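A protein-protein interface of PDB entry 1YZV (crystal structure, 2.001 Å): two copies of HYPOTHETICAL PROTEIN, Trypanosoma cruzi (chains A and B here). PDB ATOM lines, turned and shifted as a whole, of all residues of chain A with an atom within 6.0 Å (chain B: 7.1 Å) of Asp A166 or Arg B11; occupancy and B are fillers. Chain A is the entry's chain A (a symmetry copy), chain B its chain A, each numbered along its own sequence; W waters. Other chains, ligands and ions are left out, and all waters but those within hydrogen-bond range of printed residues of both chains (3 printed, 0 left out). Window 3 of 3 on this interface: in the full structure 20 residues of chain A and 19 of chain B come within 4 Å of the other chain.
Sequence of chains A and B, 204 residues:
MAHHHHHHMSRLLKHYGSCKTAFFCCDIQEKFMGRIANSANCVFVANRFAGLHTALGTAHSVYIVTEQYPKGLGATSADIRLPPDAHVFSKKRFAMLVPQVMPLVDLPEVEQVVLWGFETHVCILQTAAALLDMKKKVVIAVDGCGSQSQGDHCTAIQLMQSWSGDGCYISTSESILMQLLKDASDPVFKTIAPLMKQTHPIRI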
ATOM      1  N   ALA A 128       2.641   1.357  15.600  1.00  0.00           N
ATOM      2  CA  ALA A 128       3.919   1.272  16.302  1.00  0.00           C
ATOM      3  C   ALA A 128       4.828   0.268  15.602  1.00  0.00           C
ATOM      4  O   ALA A 128       5.999   0.559  15.378  1.00  0.00           O
ATOM      5  CB  ALA A 128       3.739   0.867  17.772  1.00  0.00           C
ATOM      6  N   ALA A 129       4.293  -0.906  15.298  1.00  0.00           N
ATOM      7  CA  ALA A 129       5.063  -1.924  14.635  1.00  0.00           C
ATOM      8  C   ALA A 129       5.586  -1.436  13.293  1.00  0.00           C
ATOM      9  O   ALA A 129       6.742  -1.690  12.948  1.00  0.00           O
ATOM     10  CB  ALA A 129       4.226  -3.212  14.461  1.00  0.00           C
ATOM     11  N   LEU A 132       8.348   0.989  13.737  1.00  0.00           N
ATOM     12  CA  LEU A 132       9.569   0.307  14.121  1.00  0.00           C
ATOM     13  C   LEU A 132      10.230  -0.309  12.897  1.00  0.00           C
ATOM     14  O   LEU A 132      11.458  -0.287  12.790  1.00  0.00           O
ATOM     15  CB  LEU A 132       9.316  -0.762  15.163  1.00  0.00           C
ATOM     16  CG  LEU A 132       9.081  -0.318  16.617  1.00  0.00           C
ATOM     17  CD1 LEU A 132       8.858  -1.551  17.452  1.00  0.00           C
ATOM     18  CD2 LEU A 132      10.284   0.504  17.119  1.00  0.00           C
ATOM     19  N   ASP A 133       9.429  -0.820  11.974  1.00  0.00           N
ATOM     20  CA  ASP A 133       9.972  -1.299  10.718  1.00  0.00           C
ATOM     21  C   ASP A 133      10.676  -0.220   9.921  1.00  0.00           C
ATOM     22  O   ASP A 133      11.533  -0.555   9.131  1.00  0.00           O
ATOM     23  CB  ASP A 133       8.894  -1.921   9.836  1.00  0.00           C
ATOM     24  CG  ASP A 133       8.477  -3.279  10.317  1.00  0.00           C
ATOM     25  OD1 ASP A 133       9.298  -3.922  11.013  1.00  0.00           O
ATOM     26  OD2 ASP A 133       7.341  -3.712   9.987  1.00  0.00           O
ATOM     27  N   LYS A 136      12.036   4.207  13.076  1.00  0.00           N
ATOM     28  CA  LYS A 136      11.704   5.421  13.796  1.00  0.00           C
ATOM     29  C   LYS A 136      11.583   5.099  15.297  1.00  0.00           C
ATOM     30  O   LYS A 136      11.227   3.987  15.674  1.00  0.00           O
ATOM     31  CB  LYS A 136      10.387   6.000  13.279  1.00  0.00           C
ATOM     32  CG  LYS A 136      10.310   6.257  11.761  1.00  0.00           C
ATOM     33  CD  LYS A 136      11.268   7.338  11.334  1.00  0.00           C
ATOM     34  CE  LYS A 136      11.166   7.652   9.853  1.00  0.00           C
ATOM     35  NZ  LYS A 136      12.021   8.857   9.502  1.00  0.00           N
ATOM     36  N   TRP A 163       8.913  -3.838  23.624  1.00  0.00           N
ATOM     37  CA  TRP A 163       9.705  -3.429  22.443  1.00  0.00           C
ATOM     38  C   TRP A 163      10.701  -2.227  22.638  1.00  0.00           C
ATOM     39  O   TRP A 163      11.228  -1.628  21.642  1.00  0.00           O
ATOM     40  CB  TRP A 163       8.778  -3.080  21.307  1.00  0.00           C
ATOM     41  CG  TRP A 163       7.795  -4.099  20.914  1.00  0.00           C
ATOM     42  CD1 TRP A 163       7.919  -5.441  21.015  1.00  0.00           C
ATOM     43  CD2 TRP A 163       6.691  -3.868  20.043  1.00  0.00           C
ATOM     44  NE1 TRP A 163       6.845  -6.061  20.436  1.00  0.00           N
ATOM     45  CE2 TRP A 163       6.151  -5.126  19.714  1.00  0.00           C
ATOM     46  CE3 TRP A 163       6.100  -2.714  19.510  1.00  0.00           C
ATOM     47  CZ2 TRP A 163       4.984  -5.252  18.994  1.00  0.00           C
ATOM     48  CZ3 TRP A 163       4.961  -2.864  18.725  1.00  0.00           C
ATOM     49  CH2 TRP A 163       4.458  -4.126  18.438  1.00  0.00           C
ATOM     50  N   SER A 164      10.901  -1.845  23.897  1.00  0.00           N
ATOM     51  CA  SER A 164      11.836  -0.728  24.276  1.00  0.00           C
ATOM     52  C   SER A 164      13.230  -0.844  23.611  1.00  0.00           C
ATOM     53  O   SER A 164      13.856   0.143  23.189  1.00  0.00           O
ATOM     54  CB  SER A 164      11.952  -0.699  25.835  1.00  0.00           C
ATOM     55  OG  SER A 164      12.439   0.547  26.323  1.00  0.00           O
ATOM     56  N   GLY A 165      13.718  -2.067  23.533  1.00  0.00           N
ATOM     57  CA  GLY A 165      15.044  -2.334  22.985  1.00  0.00           C
ATOM     58  C   GLY A 165      15.188  -1.837  21.572  1.00  0.00           C
ATOM     59  O   GLY A 165      16.277  -1.399  21.160  1.00  0.00           O
ATOM     60  N   ASP A 166      14.075  -1.842  20.842  1.00  0.00           N
ATOM     61  CA  ASP A 166      14.054  -1.498  19.430  1.00  0.00           C
ATOM     62  C   ASP A 166      13.538  -0.119  19.140  1.00  0.00           C
ATOM     63  O   ASP A 166      13.422   0.223  17.944  1.00  0.00           O
ATOM     64  CB  ASP A 166      13.208  -2.516  18.677  1.00  0.00           C
ATOM     65  CG  ASP A 166      13.907  -3.883  18.564  1.00  0.00           C
ATOM     66  OD1 ASP A 166      15.163  -3.981  18.736  1.00  0.00           O
ATOM     67  OD2 ASP A 166      13.177  -4.859  18.364  1.00  0.00           O
ATOM     68  N   GLY A 167      13.327   0.729  20.177  1.00  0.00           N
ATOM     69  CA  GLY A 167      12.889   2.081  19.913  1.00  0.00           C
ATOM     70  C   GLY A 167      11.402   2.413  20.034  1.00  0.00           C
ATOM     71  O   GLY A 167      11.032   3.511  19.703  1.00  0.00           O
ATOM     72  N   CYS A 168      10.597   1.541  20.648  1.00  0.00           N
ATOM     73  CA  CYS A 168       9.231   1.845  20.994  1.00  0.00           C
ATOM     74  C   CYS A 168       9.127   1.743  22.503  1.00  0.00           C
ATOM     75  O   CYS A 168       9.469   0.718  23.069  1.00  0.00           O
ATOM     76  CB  CYS A 168       8.284   0.829  20.388  1.00  0.00           C
ATOM     77  SG  CYS A 168       6.582   0.950  20.969  1.00  0.00           S
ATOM     78  N   SER B  10       9.521 -10.260  11.765  1.00  0.00           N
ATOM     79  CA  SER B  10       8.286  -9.440  11.945  1.00  0.00           C
ATOM     80  C   SER B  10       7.990  -9.488  13.421  1.00  0.00           C
ATOM     81  O   SER B  10       8.127 -10.537  14.029  1.00  0.00           O
ATOM     82  CB  SER B  10       7.159 -10.058  11.126  1.00  0.00           C
ATOM     83  OG  SER B  10       5.939  -9.359  11.303  1.00  0.00           O
ATOM     84  N   ARG B  11       7.610  -8.382  14.037  1.00  0.00           N
ATOM     85  CA  ARG B  11       7.305  -8.497  15.436  1.00  0.00           C
ATOM     86  C   ARG B  11       5.896  -9.000  15.754  1.00  0.00           C
ATOM     87  O   ARG B  11       5.732  -9.759  16.676  1.00  0.00           O
ATOM     88  CB  ARG B  11       7.652  -7.233  16.211  1.00  0.00           C
ATOM     89  CG  ARG B  11       6.893  -6.085  15.885  1.00  0.00           C
ATOM     90  CD  ARG B  11       7.473  -4.929  16.644  1.00  0.00           C
ATOM     91  NE  ARG B  11       8.823  -4.573  16.196  1.00  0.00           N
ATOM     92  CZ  ARG B  11       9.947  -4.842  16.859  1.00  0.00           C
ATOM     93  NH1 ARG B  11       9.943  -5.429  18.052  1.00  0.00           N
ATOM     94  NH2 ARG B  11      11.084  -4.413  16.357  1.00  0.00           N
ATOM     95  N   LEU B  12       4.931  -8.705  14.895  1.00  0.00           N
ATOM     96  CA  LEU B  12       3.575  -9.181  15.049  1.00  0.00           C
ATOM     97  C   LEU B  12       3.364 -10.321  14.067  1.00  0.00           C
ATOM     98  O   LEU B  12       4.226 -10.566  13.210  1.00  0.00           O
ATOM     99  CB  LEU B  12       2.607  -8.049  14.750  1.00  0.00           C
ATOM    100  CG  LEU B  12       2.639  -6.851  15.723  1.00  0.00           C
ATOM    101  CD1 LEU B  12       1.760  -5.776  15.194  1.00  0.00           C
ATOM    102  CD2 LEU B  12       2.263  -7.269  17.123  1.00  0.00           C
ATOM    103  N   LEU B  13       2.204 -10.981  14.155  1.00  0.00           N
ATOM    104  CA  LEU B  13       1.835 -11.998  13.175  1.00  0.00           C
ATOM    105  C   LEU B  13       1.857 -11.357  11.787  1.00  0.00           C
ATOM    106  O   LEU B  13       1.539 -10.184  11.635  1.00  0.00           O
ATOM    107  CB  LEU B  13       0.431 -12.523  13.455  1.00  0.00           C
ATOM    108  CG  LEU B  13       0.280 -13.375  14.713  1.00  0.00           C
ATOM    109  CD1 LEU B  13      -1.184 -13.469  15.074  1.00  0.00           C
ATOM    110  CD2 LEU B  13       0.887 -14.759  14.508  1.00  0.00           C
ATOM    111  N   LYS B  14       2.336 -12.103  10.812  1.00  0.00           N
ATOM    112  CA  LYS B  14       2.255 -11.717   9.407  1.00  0.00           C
ATOM    113  C   LYS B  14       0.814 -11.889   8.924  1.00  0.00           C
ATOM    114  O   LYS B  14      -0.019 -12.629   9.537  1.00  0.00           O
ATOM    115  CB  LYS B  14       3.173 -12.592   8.554  1.00  0.00           C
ATOM    116  CG  LYS B  14       4.675 -12.371   8.833  1.00  0.00           C
ATOM    117  CD  LYS B  14       5.575 -13.191   7.914  1.00  0.00           C
ATOM    118  CE  LYS B  14       7.055 -12.905   8.179  1.00  0.00           C
ATOM    119  NZ  LYS B  14       7.967 -13.874   7.474  1.00  0.00           N
ATOM    120  N   LYS B 137       7.264 -18.493  15.375  1.00  0.00           N
ATOM    121  CA  LYS B 137       6.630 -17.374  16.074  1.00  0.00           C
ATOM    122  C   LYS B 137       5.439 -17.946  16.791  1.00  0.00           C
ATOM    123  O   LYS B 137       4.746 -18.827  16.265  1.00  0.00           O
ATOM    124  CB  LYS B 137       6.166 -16.295  15.064  1.00  0.00           C
ATOM    125  CG  LYS B 137       5.432 -15.067  15.739  1.00  0.00           C
ATOM    126  CD  LYS B 137       5.021 -14.012  14.694  1.00  0.00           C
ATOM    127  CE  LYS B 137       6.203 -13.107  14.254  1.00  0.00           C
ATOM    128  NZ  LYS B 137       6.047 -12.641  12.820  1.00  0.00           N
ATOM    129  N   VAL B 139       2.136 -16.791  19.421  1.00  0.00           N
ATOM    130  CA  VAL B 139       1.375 -15.717  20.041  1.00  0.00           C
ATOM    131  C   VAL B 139       0.350 -16.336  20.941  1.00  0.00           C
ATOM    132  O   VAL B 139      -0.404 -17.237  20.499  1.00  0.00           O
ATOM    133  CB  VAL B 139       0.704 -14.836  18.968  1.00  0.00           C
ATOM    134  CG1 VAL B 139       0.036 -13.591  19.615  1.00  0.00           C
ATOM    135  CG2 VAL B 139       1.749 -14.424  18.002  1.00  0.00           C
ATOM    136  N   SER B 164       9.498 -12.197  24.298  1.00  0.00           N
ATOM    137  CA  SER B 164       9.221 -11.405  23.048  1.00  0.00           C
ATOM    138  C   SER B 164      10.431 -11.342  22.083  1.00  0.00           C
ATOM    139  O   SER B 164      10.307 -11.405  20.848  1.00  0.00           O
ATOM    140  CB  SER B 164       8.760  -9.973  23.473  1.00  0.00           C
ATOM    141  OG  SER B 164       8.067  -9.291  22.431  1.00  0.00           O
ATOM    142  N   GLY B 167      10.565 -14.304  19.740  1.00  0.00           N
ATOM    143  CA  GLY B 167       9.446 -14.718  18.924  1.00  0.00           C
ATOM    144  C   GLY B 167       8.210 -15.302  19.606  1.00  0.00           C
ATOM    145  O   GLY B 167       7.330 -15.747  18.914  1.00  0.00           O
ATOM    146  N   TYR B 169       5.143 -13.793  21.935  1.00  0.00           N
ATOM    147  CA  TYR B 169       4.489 -12.734  22.699  1.00  0.00           C
ATOM    148  C   TYR B 169       3.033 -12.994  23.042  1.00  0.00           C
ATOM    149  O   TYR B 169       2.415 -13.985  22.602  1.00  0.00           O
ATOM    150  CB  TYR B 169       4.588 -11.444  21.956  1.00  0.00           C
ATOM    151  CG  TYR B 169       3.812 -11.441  20.692  1.00  0.00           C
ATOM    152  CD1 TYR B 169       4.431 -11.795  19.497  1.00  0.00           C
ATOM    153  CD2 TYR B 169       2.554 -10.770  20.618  1.00  0.00           C
ATOM    154  CE1 TYR B 169       3.735 -11.722  18.303  1.00  0.00           C
ATOM    155  CE2 TYR B 169       1.849 -10.689  19.433  1.00  0.00           C
ATOM    156  CZ  TYR B 169       2.414 -11.236  18.272  1.00  0.00           C
ATOM    157  OH  TYR B 169       1.772 -11.090  17.033  1.00  0.00           O
ATOM    158  N   GLN B 179      -4.465  -8.453  13.541  1.00  0.00           N
ATOM    159  CA  GLN B 179      -3.069  -8.681  13.094  1.00  0.00           C
ATOM    160  C   GLN B 179      -2.952  -9.521  11.820  1.00  0.00           C
ATOM    161  O   GLN B 179      -2.122  -9.233  10.940  1.00  0.00           O
ATOM    162  CB  GLN B 179      -2.204  -9.338  14.185  1.00  0.00           C
ATOM    163  CG  GLN B 179      -1.833  -8.405  15.321  1.00  0.00           C
ATOM    164  CD  GLN B 179      -1.262  -9.180  16.528  1.00  0.00           C
ATOM    165  OE1 GLN B 179      -0.422 -10.033  16.353  1.00  0.00           O
ATOM    166  NE2 GLN B 179      -1.761  -8.899  17.718  1.00  0.00           N
HETATM  167  O   HOH W   1       6.878  -9.020  19.773  1.00  0.00           O
HETATM  168  O   HOH W   2       8.075  -3.980  13.526  1.00  0.00           O
HETATM  169  O   HOH W   3      10.662  -4.104  13.879  1.00  0.00           O
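Arg B11 touches three residues of chain A.
Of the printed residues of chain A, Leu B12 touches Ala A129 (3.6 Å) and Trp A163 (3.9 Å).
Printed residues of chain B within 4 Å of Trp A163: Arg B11 (3.3 Å), Leu B12 (3.9 Å) and Ser B164 (3.99 Å).
Printed residues of chain B within 4 Å of Ala A129: Leu B12.
Of the printed residues of chain A, Ser B164 touches Trp A163.
Of the printed residues of chain B, Leu A132 touches Arg B11 (3.3 Å).
Gly B167 touches none of the printed residues of chain A.
The nearest printed residue of chain B that does not touch Asp A166 is Ser B164 (7.6 Å).
The nearest printed residue of chain A that does not touch Leu B12 is Ala A128 (6.8 Å).
Among the printed residues, pairs that only touch across the chains: Leu A132 with Arg B11 (3.3 Å), Trp A163 with Arg B11 (3.3 Å), Ala A129 with Leu B12 (3.6 Å), Trp A163 with Leu B12 (3.9 Å) and Trp A163 with Ser B164 (3.99 Å).
The side-chain hydroxyl of Ser B10 sits at hydrogen-bond distance from the backbone carbonyl oxygen of Leu B12 (2.8 Å).
The backbone carbonyl oxygen (O) of Leu B12 is in hydrogen-bond range of the side-chain amino group (NZ) of Lys B137 (2.8 Å).
N of Cys A168 sits at hydrogen-bond distance from O of Trp A163, 3.4 Å away.
2 positions are printed for both chains.
The side-chain carboxylate of Asp A166 lies within salt-bridge range of the guanidinium group of Arg B11.
Hydrophobic or aromatic side chains of chain A that line the printed part of chain B: Ala A129, Leu A132 and Trp A163.
Printed residues of chain B that touch a printed residue of chain A: Arg B11, Leu B12 and Ser B164.
Among the printed residues, 6 pairs touch across the chains.
Among the printed residues, Asp or Glu carboxylates within 4 Å of a Lys or Arg side-chain nitrogen of the other chain: Asp A166 with Arg B11 (2.9 Å).
Water W3 bridges NH2 of Arg B11 (2.5 Å) and OD1 of Asp A133 (3.2 Å).
Water W2 lies within hydrogen-bond range of O of Ala A129 (2.7 Å), OD1 of Asp A133 (2.8 Å) and NE of Arg B11 (2.8 Å).
Water W1 lies within hydrogen-bond range of the side-chain hydroxyl (OG) of Ser B164 (2.9 Å), the indole nitrogen (NE1) of Trp A163 (3.0 Å) and the backbone carbonyl oxygen (O) of Arg B11 (3.4 Å).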
